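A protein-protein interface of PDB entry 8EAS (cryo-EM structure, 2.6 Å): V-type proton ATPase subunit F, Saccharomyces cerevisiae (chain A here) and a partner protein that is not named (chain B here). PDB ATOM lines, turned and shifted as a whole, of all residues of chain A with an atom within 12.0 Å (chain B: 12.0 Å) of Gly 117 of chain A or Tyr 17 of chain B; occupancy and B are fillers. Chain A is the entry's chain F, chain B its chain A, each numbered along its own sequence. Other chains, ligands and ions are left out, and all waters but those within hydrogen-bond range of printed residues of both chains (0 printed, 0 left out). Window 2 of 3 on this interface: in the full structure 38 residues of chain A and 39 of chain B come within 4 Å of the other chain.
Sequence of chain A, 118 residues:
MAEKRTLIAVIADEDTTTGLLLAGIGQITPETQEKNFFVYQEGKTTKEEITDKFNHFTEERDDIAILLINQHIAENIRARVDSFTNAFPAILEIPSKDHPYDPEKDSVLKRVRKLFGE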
ATOM      1  N   SER A 107     -35.392 -12.693 -34.119  1.00  0.00           N
ATOM      2  CA  SER A 107     -35.151 -12.765 -32.682  1.00  0.00           C
ATOM      3  C   SER A 107     -34.034 -11.822 -32.253  1.00  0.00           C
ATOM      4  O   SER A 107     -34.082 -11.259 -31.155  1.00  0.00           O
ATOM      5  CB  SER A 107     -34.819 -14.200 -32.277  1.00  0.00           C
ATOM      6  OG  SER A 107     -35.919 -15.061 -32.511  1.00  0.00           O
ATOM      7  N   VAL A 108     -33.025 -11.645 -33.107  1.00  0.00           N
ATOM      8  CA  VAL A 108     -31.895 -10.782 -32.770  1.00  0.00           C
ATOM      9  C   VAL A 108     -32.352  -9.340 -32.604  1.00  0.00           C
ATOM     10  O   VAL A 108     -31.926  -8.637 -31.678  1.00  0.00           O
ATOM     11  CB  VAL A 108     -30.800 -10.907 -33.844  1.00  0.00           C
ATOM     12  CG1 VAL A 108     -29.616 -10.033 -33.495  1.00  0.00           C
ATOM     13  CG2 VAL A 108     -30.378 -12.351 -33.989  1.00  0.00           C
ATOM     14  N   LEU A 109     -33.212  -8.869 -33.507  1.00  0.00           N
ATOM     15  CA  LEU A 109     -33.681  -7.491 -33.433  1.00  0.00           C
ATOM     16  C   LEU A 109     -34.517  -7.262 -32.181  1.00  0.00           C
ATOM     17  O   LEU A 109     -34.409  -6.212 -31.540  1.00  0.00           O
ATOM     18  CB  LEU A 109     -34.469  -7.143 -34.693  1.00  0.00           C
ATOM     19  CG  LEU A 109     -33.685  -7.371 -35.987  1.00  0.00           C
ATOM     20  CD1 LEU A 109     -34.462  -6.872 -37.191  1.00  0.00           C
ATOM     21  CD2 LEU A 109     -32.318  -6.709 -35.917  1.00  0.00           C
ATOM     22  N   LYS A 110     -35.348  -8.236 -31.806  1.00  0.00           N
ATOM     23  CA  LYS A 110     -36.113  -8.104 -30.570  1.00  0.00           C
ATOM     24  C   LYS A 110     -35.201  -8.148 -29.348  1.00  0.00           C
ATOM     25  O   LYS A 110     -35.447  -7.452 -28.354  1.00  0.00           O
ATOM     26  CB  LYS A 110     -37.182  -9.193 -30.494  1.00  0.00           C
ATOM     27  CG  LYS A 110     -38.326  -8.993 -31.477  1.00  0.00           C
ATOM     28  CD  LYS A 110     -39.470  -9.956 -31.213  1.00  0.00           C
ATOM     29  CE  LYS A 110     -39.116 -11.369 -31.641  1.00  0.00           C
ATOM     30  NZ  LYS A 110     -40.328 -12.226 -31.763  1.00  0.00           N
ATOM     31  N   ARG A 111     -34.134  -8.946 -29.398  1.00  0.00           N
ATOM     32  CA  ARG A 111     -33.221  -8.981 -28.261  1.00  0.00           C
ATOM     33  C   ARG A 111     -32.485  -7.652 -28.122  1.00  0.00           C
ATOM     34  O   ARG A 111     -32.237  -7.186 -27.004  1.00  0.00           O
ATOM     35  CB  ARG A 111     -32.234 -10.139 -28.402  1.00  0.00           C
ATOM     36  CG  ARG A 111     -31.242 -10.228 -27.254  1.00  0.00           C
ATOM     37  CD  ARG A 111     -31.990 -10.571 -25.969  1.00  0.00           C
ATOM     38  NE  ARG A 111     -31.119 -10.709 -24.808  1.00  0.00           N
ATOM     39  CZ  ARG A 111     -30.738  -9.701 -24.036  1.00  0.00           C
ATOM     40  NH1 ARG A 111     -31.119  -8.459 -24.282  1.00  0.00           N
ATOM     41  NH2 ARG A 111     -29.957  -9.946 -22.987  1.00  0.00           N
ATOM     42  N   VAL A 112     -32.128  -7.029 -29.248  1.00  0.00           N
ATOM     43  CA  VAL A 112     -31.542  -5.688 -29.206  1.00  0.00           C
ATOM     44  C   VAL A 112     -32.559  -4.677 -28.686  1.00  0.00           C
ATOM     45  O   VAL A 112     -32.215  -3.766 -27.921  1.00  0.00           O
ATOM     46  CB  VAL A 112     -30.996  -5.293 -30.590  1.00  0.00           C
ATOM     47  CG1 VAL A 112     -30.613  -3.824 -30.612  1.00  0.00           C
ATOM     48  CG2 VAL A 112     -29.784  -6.139 -30.930  1.00  0.00           C
ATOM     49  N   ARG A 113     -33.824  -4.824 -29.091  1.00  0.00           N
ATOM     50  CA  ARG A 113     -34.912  -4.063 -28.482  1.00  0.00           C
ATOM     51  C   ARG A 113     -34.880  -4.169 -26.963  1.00  0.00           C
ATOM     52  O   ARG A 113     -35.097  -3.176 -26.258  1.00  0.00           O
ATOM     53  CB  ARG A 113     -36.261  -4.575 -28.988  1.00  0.00           C
ATOM     54  CG  ARG A 113     -36.776  -4.049 -30.313  1.00  0.00           C
ATOM     55  CD  ARG A 113     -37.022  -2.553 -30.239  1.00  0.00           C
ATOM     56  NE  ARG A 113     -37.368  -1.992 -31.541  1.00  0.00           N
ATOM     57  CZ  ARG A 113     -37.621  -0.709 -31.766  1.00  0.00           C
ATOM     58  NH1 ARG A 113     -37.440   0.208 -30.828  1.00  0.00           N
ATOM     59  NH2 ARG A 113     -38.078  -0.339 -32.959  1.00  0.00           N
ATOM     60  N   LYS A 114     -34.633  -5.376 -26.448  1.00  0.00           N
ATOM     61  CA  LYS A 114     -34.646  -5.590 -25.001  1.00  0.00           C
ATOM     62  C   LYS A 114     -33.663  -4.682 -24.271  1.00  0.00           C
ATOM     63  O   LYS A 114     -33.946  -4.243 -23.149  1.00  0.00           O
ATOM     64  CB  LYS A 114     -34.345  -7.054 -24.676  1.00  0.00           C
ATOM     65  CG  LYS A 114     -35.374  -8.030 -25.205  1.00  0.00           C
ATOM     66  CD  LYS A 114     -36.713  -7.784 -24.538  1.00  0.00           C
ATOM     67  CE  LYS A 114     -36.694  -8.208 -23.077  1.00  0.00           C
ATOM     68  NZ  LYS A 114     -38.032  -8.036 -22.446  1.00  0.00           N
ATOM     69  N   LEU A 115     -32.511  -4.389 -24.875  1.00  0.00           N
ATOM     70  CA  LEU A 115     -31.551  -3.489 -24.246  1.00  0.00           C
ATOM     71  C   LEU A 115     -31.993  -2.033 -24.275  1.00  0.00           C
ATOM     72  O   LEU A 115     -31.387  -1.207 -23.582  1.00  0.00           O
ATOM     73  CB  LEU A 115     -30.183  -3.610 -24.918  1.00  0.00           C
ATOM     74  CG  LEU A 115     -29.401  -4.907 -24.723  1.00  0.00           C
ATOM     75  CD1 LEU A 115     -28.045  -4.795 -25.395  1.00  0.00           C
ATOM     76  CD2 LEU A 115     -29.244  -5.220 -23.246  1.00  0.00           C
ATOM     77  N   PHE A 116     -33.023  -1.699 -25.056  1.00  0.00           N
ATOM     78  CA  PHE A 116     -33.470  -0.315 -25.221  1.00  0.00           C
ATOM     79  C   PHE A 116     -32.327   0.581 -25.691  1.00  0.00           C
ATOM     80  O   PHE A 116     -32.184   1.723 -25.250  1.00  0.00           O
ATOM     81  CB  PHE A 116     -34.096   0.225 -23.933  1.00  0.00           C
ATOM     82  CG  PHE A 116     -35.477  -0.295 -23.664  1.00  0.00           C
ATOM     83  CD1 PHE A 116     -36.246  -0.822 -24.688  1.00  0.00           C
ATOM     84  CD2 PHE A 116     -36.004  -0.268 -22.383  1.00  0.00           C
ATOM     85  CE1 PHE A 116     -37.518  -1.303 -24.443  1.00  0.00           C
ATOM     86  CE2 PHE A 116     -37.275  -0.749 -22.131  1.00  0.00           C
ATOM     87  CZ  PHE A 116     -38.032  -1.268 -23.162  1.00  0.00           C
ATOM     88  N   GLY A 117     -31.506   0.057 -26.592  1.00  0.00           N
ATOM     89  CA  GLY A 117     -30.369   0.794 -27.104  1.00  0.00           C
ATOM     90  C   GLY A 117     -29.192  -0.095 -27.445  1.00  0.00           C
ATOM     91  O   GLY A 117     -29.202  -1.289 -27.154  1.00  0.00           O
ATOM     92  N   ASP B  14     -19.212   3.614 -22.929  1.00  0.00           N
ATOM     93  CA  ASP B  14     -18.473   2.454 -23.410  1.00  0.00           C
ATOM     94  C   ASP B  14     -18.590   2.305 -24.924  1.00  0.00           C
ATOM     95  O   ASP B  14     -19.597   2.684 -25.522  1.00  0.00           O
ATOM     96  CB  ASP B  14     -18.962   1.184 -22.714  1.00  0.00           C
ATOM     97  CG  ASP B  14     -20.474   1.105 -22.645  1.00  0.00           C
ATOM     98  OD1 ASP B  14     -21.144   1.997 -23.205  1.00  0.00           O
ATOM     99  OD2 ASP B  14     -20.993   0.148 -22.030  1.00  0.00           O
ATOM    100  N   GLU B  15     -17.546   1.748 -25.539  1.00  0.00           N
ATOM    101  CA  GLU B  15     -17.524   1.547 -26.982  1.00  0.00           C
ATOM    102  C   GLU B  15     -18.178   0.242 -27.410  1.00  0.00           C
ATOM    103  O   GLU B  15     -18.256  -0.023 -28.615  1.00  0.00           O
ATOM    104  CB  GLU B  15     -16.084   1.594 -27.493  1.00  0.00           C
ATOM    105  CG  GLU B  15     -15.235   0.410 -27.055  1.00  0.00           C
ATOM    106  CD  GLU B  15     -14.622   0.602 -25.678  1.00  0.00           C
ATOM    107  OE1 GLU B  15     -15.077   1.498 -24.938  1.00  0.00           O
ATOM    108  OE2 GLU B  15     -13.689  -0.152 -25.333  1.00  0.00           O
ATOM    109  N   GLN B  16     -18.643  -0.579 -26.463  1.00  0.00           N
ATOM    110  CA  GLN B  16     -19.285  -1.840 -26.823  1.00  0.00           C
ATOM    111  C   GLN B  16     -20.558  -1.613 -27.626  1.00  0.00           C
ATOM    112  O   GLN B  16     -20.900  -2.428 -28.491  1.00  0.00           O
ATOM    113  CB  GLN B  16     -19.589  -2.652 -25.566  1.00  0.00           C
ATOM    114  N   TYR B  17     -21.272  -0.516 -27.361  1.00  0.00           N
ATOM    115  CA  TYR B  17     -22.474  -0.217 -28.133  1.00  0.00           C
ATOM    116  C   TYR B  17     -22.131   0.166 -29.567  1.00  0.00           C
ATOM    117  O   TYR B  17     -22.888  -0.139 -30.494  1.00  0.00           O
ATOM    118  CB  TYR B  17     -23.271   0.889 -27.448  1.00  0.00           C
ATOM    119  CG  TYR B  17     -23.990   0.420 -26.209  1.00  0.00           C
ATOM    120  CD1 TYR B  17     -25.242  -0.172 -26.292  1.00  0.00           C
ATOM    121  CD2 TYR B  17     -23.414   0.557 -24.955  1.00  0.00           C
ATOM    122  CE1 TYR B  17     -25.902  -0.608 -25.160  1.00  0.00           C
ATOM    123  CE2 TYR B  17     -24.067   0.126 -23.818  1.00  0.00           C
ATOM    124  CZ  TYR B  17     -25.311  -0.455 -23.927  1.00  0.00           C
ATOM    125  OH  TYR B  17     -25.963  -0.887 -22.796  1.00  0.00           O
ATOM    126  N   LEU B  18     -20.996   0.837 -29.770  1.00  0.00           N
ATOM    127  CA  LEU B  18     -20.552   1.135 -31.128  1.00  0.00           C
ATOM    128  C   LEU B  18     -20.271  -0.146 -31.904  1.00  0.00           C
ATOM    129  O   LEU B  18     -20.640  -0.269 -33.081  1.00  0.00           O
ATOM    130  CB  LEU B  18     -19.310   2.022 -31.081  1.00  0.00           C
ATOM    131  CG  LEU B  18     -18.725   2.499 -32.407  1.00  0.00           C
ATOM    132  CD1 LEU B  18     -19.719   3.371 -33.153  1.00  0.00           C
ATOM    133  CD2 LEU B  18     -17.431   3.244 -32.154  1.00  0.00           C
ATOM    134  N   ARG B  19     -19.628  -1.120 -31.258  1.00  0.00           N
ATOM    135  CA  ARG B  19     -19.411  -2.407 -31.906  1.00  0.00           C
ATOM    136  C   ARG B  19     -20.723  -3.146 -32.127  1.00  0.00           C
ATOM    137  O   ARG B  19     -20.862  -3.870 -33.118  1.00  0.00           O
ATOM    138  CB  ARG B  19     -18.446  -3.257 -31.085  1.00  0.00           C
ATOM    139  CG  ARG B  19     -17.031  -2.700 -31.035  1.00  0.00           C
ATOM    140  CD  ARG B  19     -16.067  -3.710 -30.444  1.00  0.00           C
ATOM    141  NE  ARG B  19     -15.881  -4.845 -31.340  1.00  0.00           N
ATOM    142  CZ  ARG B  19     -16.379  -6.055 -31.132  1.00  0.00           C
ATOM    143  NH1 ARG B  19     -17.087  -6.333 -30.049  1.00  0.00           N
ATOM    144  NH2 ARG B  19     -16.163  -7.009 -32.032  1.00  0.00           N
ATOM    145  N   LEU B  20     -21.695  -2.978 -31.228  1.00  0.00           N
ATOM    146  CA  LEU B  20     -23.016  -3.551 -31.464  1.00  0.00           C
ATOM    147  C   LEU B  20     -23.658  -2.952 -32.708  1.00  0.00           C
ATOM    148  O   LEU B  20     -24.275  -3.667 -33.504  1.00  0.00           O
ATOM    149  CB  LEU B  20     -23.913  -3.337 -30.245  1.00  0.00           C
ATOM    150  CG  LEU B  20     -25.352  -3.834 -30.388  1.00  0.00           C
ATOM    151  CD1 LEU B  20     -25.376  -5.291 -30.806  1.00  0.00           C
ATOM    152  CD2 LEU B  20     -26.122  -3.636 -29.096  1.00  0.00           C
ATOM    153  N   ILE B  21     -23.524  -1.638 -32.888  1.00  0.00           N
ATOM    154  CA  ILE B  21     -24.062  -0.987 -34.081  1.00  0.00           C
ATOM    155  C   ILE B  21     -23.367  -1.509 -35.333  1.00  0.00           C
ATOM    156  O   ILE B  21     -24.011  -1.772 -36.356  1.00  0.00           O
ATOM    157  CB  ILE B  21     -23.938   0.542 -33.961  1.00  0.00           C
ATOM    158  CG1 ILE B  21     -24.818   1.059 -32.822  1.00  0.00           C
ATOM    159  CG2 ILE B  21     -24.316   1.217 -35.270  1.00  0.00           C
ATOM    160  CD1 ILE B  21     -26.280   0.706 -32.974  1.00  0.00           C
ATOM    161  N   GLU B  22     -22.043  -1.661 -35.276  1.00  0.00           N
ATOM    162  CA  GLU B  22     -21.308  -2.180 -36.427  1.00  0.00           C
ATOM    163  C   GLU B  22     -21.744  -3.603 -36.761  1.00  0.00           C
ATOM    164  O   GLU B  22     -21.937  -3.950 -37.936  1.00  0.00           O
ATOM    165  CB  GLU B  22     -19.806  -2.121 -36.145  1.00  0.00           C
ATOM    166  CG  GLU B  22     -18.916  -2.227 -37.372  1.00  0.00           C
ATOM    167  CD  GLU B  22     -18.484  -3.646 -37.662  1.00  0.00           C
ATOM    168  OE1 GLU B  22     -18.399  -4.451 -36.712  1.00  0.00           O
ATOM    169  OE2 GLU B  22     -18.220  -3.957 -38.842  1.00  0.00           O
ATOM    170  N   LEU B  23     -21.916  -4.438 -35.735  1.00  0.00           N
ATOM    171  CA  LEU B  23     -22.373  -5.803 -35.953  1.00  0.00           C
ATOM    172  C   LEU B  23     -23.781  -5.828 -36.528  1.00  0.00           C
ATOM    173  O   LEU B  23     -24.087  -6.654 -37.389  1.00  0.00           O
ATOM    174  CB  LEU B  23     -22.315  -6.591 -34.648  1.00  0.00           C
ATOM    175  CG  LEU B  23     -20.914  -6.956 -34.171  1.00  0.00           C
ATOM    176  CD1 LEU B  23     -20.994  -7.793 -32.910  1.00  0.00           C
ATOM    177  CD2 LEU B  23     -20.168  -7.691 -35.271  1.00  0.00           C
ATOM    178  N   LEU B  24     -24.658  -4.939 -36.055  1.00  0.00           N
ATOM    179  CA  LEU B  24     -26.002  -4.863 -36.613  1.00  0.00           C
ATOM    180  C   LEU B  24     -25.970  -4.433 -38.073  1.00  0.00           C
ATOM    181  O   LEU B  24     -26.763  -4.917 -38.885  1.00  0.00           O
ATOM    182  CB  LEU B  24     -26.864  -3.908 -35.793  1.00  0.00           C
ATOM    183  CG  LEU B  24     -27.511  -4.509 -34.547  1.00  0.00           C
ATOM    184  CD1 LEU B  24     -27.955  -3.411 -33.601  1.00  0.00           C
ATOM    185  CD2 LEU B  24     -28.679  -5.393 -34.943  1.00  0.00           C
ATOM    186  N   SER B  25     -25.065  -3.522 -38.424  1.00  0.00           N
ATOM    187  CA  SER B  25     -24.925  -3.123 -39.820  1.00  0.00           C
ATOM    188  C   SER B  25     -24.492  -4.297 -40.687  1.00  0.00           C
ATOM    189  O   SER B  25     -25.047  -4.530 -41.769  1.00  0.00           O
ATOM    190  CB  SER B  25     -23.919  -1.984 -39.940  1.00  0.00           C
ATOM    191  OG  SER B  25     -23.570  -1.790 -41.294  1.00  0.00           O
ATOM    192  N   ASN B  26     -23.485  -5.044 -40.229  1.00  0.00           N
ATOM    193  CA  ASN B  26     -23.035  -6.204 -40.995  1.00  0.00           C
ATOM    194  C   ASN B  26     -24.119  -7.271 -41.068  1.00  0.00           C
ATOM    195  O   ASN B  26     -24.269  -7.941 -42.094  1.00  0.00           O
ATOM    196  CB  ASN B  26     -21.754  -6.773 -40.392  1.00  0.00           C
ATOM    197  CG  ASN B  26     -20.613  -5.783 -40.412  1.00  0.00           C
ATOM    198  OD1 ASN B  26     -20.427  -5.055 -41.385  1.00  0.00           O
ATOM    199  ND2 ASN B  26     -19.836  -5.757 -39.341  1.00  0.00           N
ATOM    200  N   GLU B 169     -22.364 -13.436 -32.611  1.00  0.00           N
ATOM    201  CA  GLU B 169     -21.540 -12.346 -32.102  1.00  0.00           C
ATOM    202  C   GLU B 169     -22.397 -11.254 -31.477  1.00  0.00           C
ATOM    203  O   GLU B 169     -22.058 -10.722 -30.412  1.00  0.00           O
ATOM    204  CB  GLU B 169     -20.683 -11.781 -33.234  1.00  0.00           C
ATOM    205  CG  GLU B 169     -19.452 -11.027 -32.784  1.00  0.00           C
ATOM    206  CD  GLU B 169     -18.650 -10.487 -33.953  1.00  0.00           C
ATOM    207  OE1 GLU B 169     -18.942 -10.874 -35.103  1.00  0.00           O
ATOM    208  OE2 GLU B 169     -17.729  -9.675 -33.724  1.00  0.00           O
ATOM    209  N   ILE B 170     -23.516 -10.911 -32.119  1.00  0.00           N
ATOM    210  CA  ILE B 170     -24.420  -9.905 -31.569  1.00  0.00           C
ATOM    211  C   ILE B 170     -24.999 -10.381 -30.246  1.00  0.00           C
ATOM    212  O   ILE B 170     -25.081  -9.616 -29.281  1.00  0.00           O
ATOM    213  CB  ILE B 170     -25.535  -9.570 -32.578  1.00  0.00           C
ATOM    214  CG1 ILE B 170     -24.981  -8.766 -33.754  1.00  0.00           C
ATOM    215  CG2 ILE B 170     -26.647  -8.789 -31.901  1.00  0.00           C
ATOM    216  CD1 ILE B 170     -25.882  -8.770 -34.968  1.00  0.00           C
ATOM    217  N   LEU B 171     -25.413 -11.648 -30.180  1.00  0.00           N
ATOM    218  CA  LEU B 171     -25.973 -12.170 -28.937  1.00  0.00           C
ATOM    219  C   LEU B 171     -24.938 -12.176 -27.819  1.00  0.00           C
ATOM    220  O   LEU B 171     -25.251 -11.836 -26.674  1.00  0.00           O
ATOM    221  CB  LEU B 171     -26.537 -13.572 -29.163  1.00  0.00           C
ATOM    222  CG  LEU B 171     -27.853 -13.645 -29.939  1.00  0.00           C
ATOM    223  CD1 LEU B 171     -28.548 -14.969 -29.681  1.00  0.00           C
ATOM    224  CD2 LEU B 171     -28.761 -12.484 -29.573  1.00  0.00           C
ATOM    225  N   THR B 172     -23.697 -12.556 -28.131  1.00  0.00           N
ATOM    226  CA  THR B 172     -22.648 -12.548 -27.117  1.00  0.00           C
ATOM    227  C   THR B 172     -22.353 -11.133 -26.635  1.00  0.00           C
ATOM    228  O   THR B 172     -22.204 -10.898 -25.429  1.00  0.00           O
ATOM    229  CB  THR B 172     -21.382 -13.206 -27.668  1.00  0.00           C
ATOM    230  OG1 THR B 172     -21.666 -14.562 -28.031  1.00  0.00           O
ATOM    231  CG2 THR B 172     -20.273 -13.191 -26.628  1.00  0.00           C
ATOM    232  N   LEU B 173     -22.278 -10.173 -27.560  1.00  0.00           N
ATOM    233  CA  LEU B 173     -22.025  -8.790 -27.171  1.00  0.00           C
ATOM    234  C   LEU B 173     -23.174  -8.235 -26.336  1.00  0.00           C
ATOM    235  O   LEU B 173     -22.950  -7.472 -25.391  1.00  0.00           O
ATOM    236  CB  LEU B 173     -21.792  -7.933 -28.414  1.00  0.00           C
ATOM    237  CG  LEU B 173     -21.114  -6.573 -28.234  1.00  0.00           C
ATOM    238  CD1 LEU B 173     -20.324  -6.219 -29.480  1.00  0.00           C
ATOM    239  CD2 LEU B 173     -22.123  -5.485 -27.924  1.00  0.00           C
ATOM    240  N   VAL B 174     -24.412  -8.595 -26.682  1.00  0.00           N
ATOM    241  CA  VAL B 174     -25.567  -8.153 -25.907  1.00  0.00           C
ATOM    242  C   VAL B 174     -25.535  -8.765 -24.512  1.00  0.00           C
ATOM    243  O   VAL B 174     -25.847  -8.097 -23.518  1.00  0.00           O
ATOM    244  CB  VAL B 174     -26.869  -8.496 -26.654  1.00  0.00           C
ATOM    245  CG1 VAL B 174     -28.052  -8.471 -25.711  1.00  0.00           C
ATOM    246  CG2 VAL B 174     -27.084  -7.524 -27.801  1.00  0.00           C
ATOM    247  N   GLU B 175     -25.155 -10.040 -24.414  1.00  0.00           N
ATOM    248  CA  GLU B 175     -24.992 -10.667 -23.107  1.00  0.00           C
ATOM    249  C   GLU B 175     -23.919  -9.956 -22.292  1.00  0.00           C
ATOM    250  O   GLU B 175     -24.041  -9.827 -21.069  1.00  0.00           O
ATOM    251  CB  GLU B 175     -24.646 -12.146 -23.273  1.00  0.00           C
ATOM    252  CG  GLU B 175     -25.852 -13.042 -23.489  1.00  0.00           C
ATOM    253  CD  GLU B 175     -26.332 -13.689 -22.206  1.00  0.00           C
ATOM    254  OE1 GLU B 175     -25.979 -13.188 -21.117  1.00  0.00           O
ATOM    255  OE2 GLU B 175     -27.062 -14.699 -22.285  1.00  0.00           O
ATOM    256  N   THR B 176     -22.855  -9.498 -22.955  1.00  0.00           N
ATOM    257  CA  THR B 176     -21.846  -8.699 -22.267  1.00  0.00           C
ATOM    258  C   THR B 176     -22.445  -7.407 -21.725  1.00  0.00           C
ATOM    259  O   THR B 176     -22.151  -7.004 -20.593  1.00  0.00           O
ATOM    260  CB  THR B 176     -20.680  -8.398 -23.210  1.00  0.00           C
ATOM    261  OG1 THR B 176     -20.021  -9.621 -23.564  1.00  0.00           O
ATOM    262  CG2 THR B 176     -19.680  -7.459 -22.551  1.00  0.00           C
ATOM    263  N   LEU B 177     -23.294  -6.750 -22.508  1.00  0.00           N
ATOM    264  CA  LEU B 177     -23.921  -5.510 -22.069  1.00  0.00           C
ATOM    265  C   LEU B 177     -25.222  -5.779 -21.320  1.00  0.00           C
ATOM    266  O   LEU B 177     -25.963  -4.855 -20.986  1.00  0.00           O
ATOM    267  CB  LEU B 177     -24.179  -4.587 -23.261  1.00  0.00           C
ATOM    268  CG  LEU B 177     -22.930  -4.004 -23.921  1.00  0.00           C
ATOM    269  CD1 LEU B 177     -23.285  -3.257 -25.197  1.00  0.00           C
ATOM    270  CD2 LEU B 177     -22.191  -3.100 -22.953  1.00  0.00           C
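Among the printed residues, merely in contact across the chains: Arg 111 of chain A with Val 174 of chain B (3.4 Å), Val 108 of chain A with Ile 170 of chain B (3.6 Å), Leu 115 of chain A with Val 174 of chain B (3.7 Å), Gly 117 of chain A with Tyr 17 of chain B (3.9 Å) and Leu 109 of chain A with Leu 24 of chain B (3.99 Å).
Gly 117 of chain A touches just one residue of chain B: Tyr 17. Tyr 17 of chain B touches one residue of chain A. No residue of chain B comes within 4 Å of Val 112 of chain A. No residue of chain B comes within 4 Å of Phe 116 of chain A. No residue of chain A comes within 4 Å of Asp 14 of chain B. No residue of chain A comes within 4 Å of Gln 16 of chain B. No residue of chain A comes within 4 Å of Leu 18 of chain B. No residue of chain A comes within 4 Å of Ile 21 of chain B. Printed residues of chain A within 4 Å of Ile 170 of chain B: Val 108 (3.6 Å). Printed residues of chain B within 4 Å of Leu 115 of chain A: Val 174. Printed residues of chain B within 4 Å of Arg 111 of chain A: Val 174 (3.4 Å). Printed residues of chain A within 4 Å of Leu 24 of chain B: Leu 109 (3.99 Å). The nearest residue of chain B that does not touch Gly 117 of chain A is Leu 20 of chain B (4.3 Å). The nearest printed residue of chain A that does not touch Ile 170 of chain B is Val 112 of chain A (4.2 Å).
Hydrophobic or aromatic side chains of chain A that line the printed part of chain B: Val 108, Leu 109 and Leu 115. Hydrophobic or aromatic side chains of chain B that line the printed part of chain A: Tyr 17, Leu 24, Ile 170 and Val 174. Among the printed residues, 5 pairs touch across the chains.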
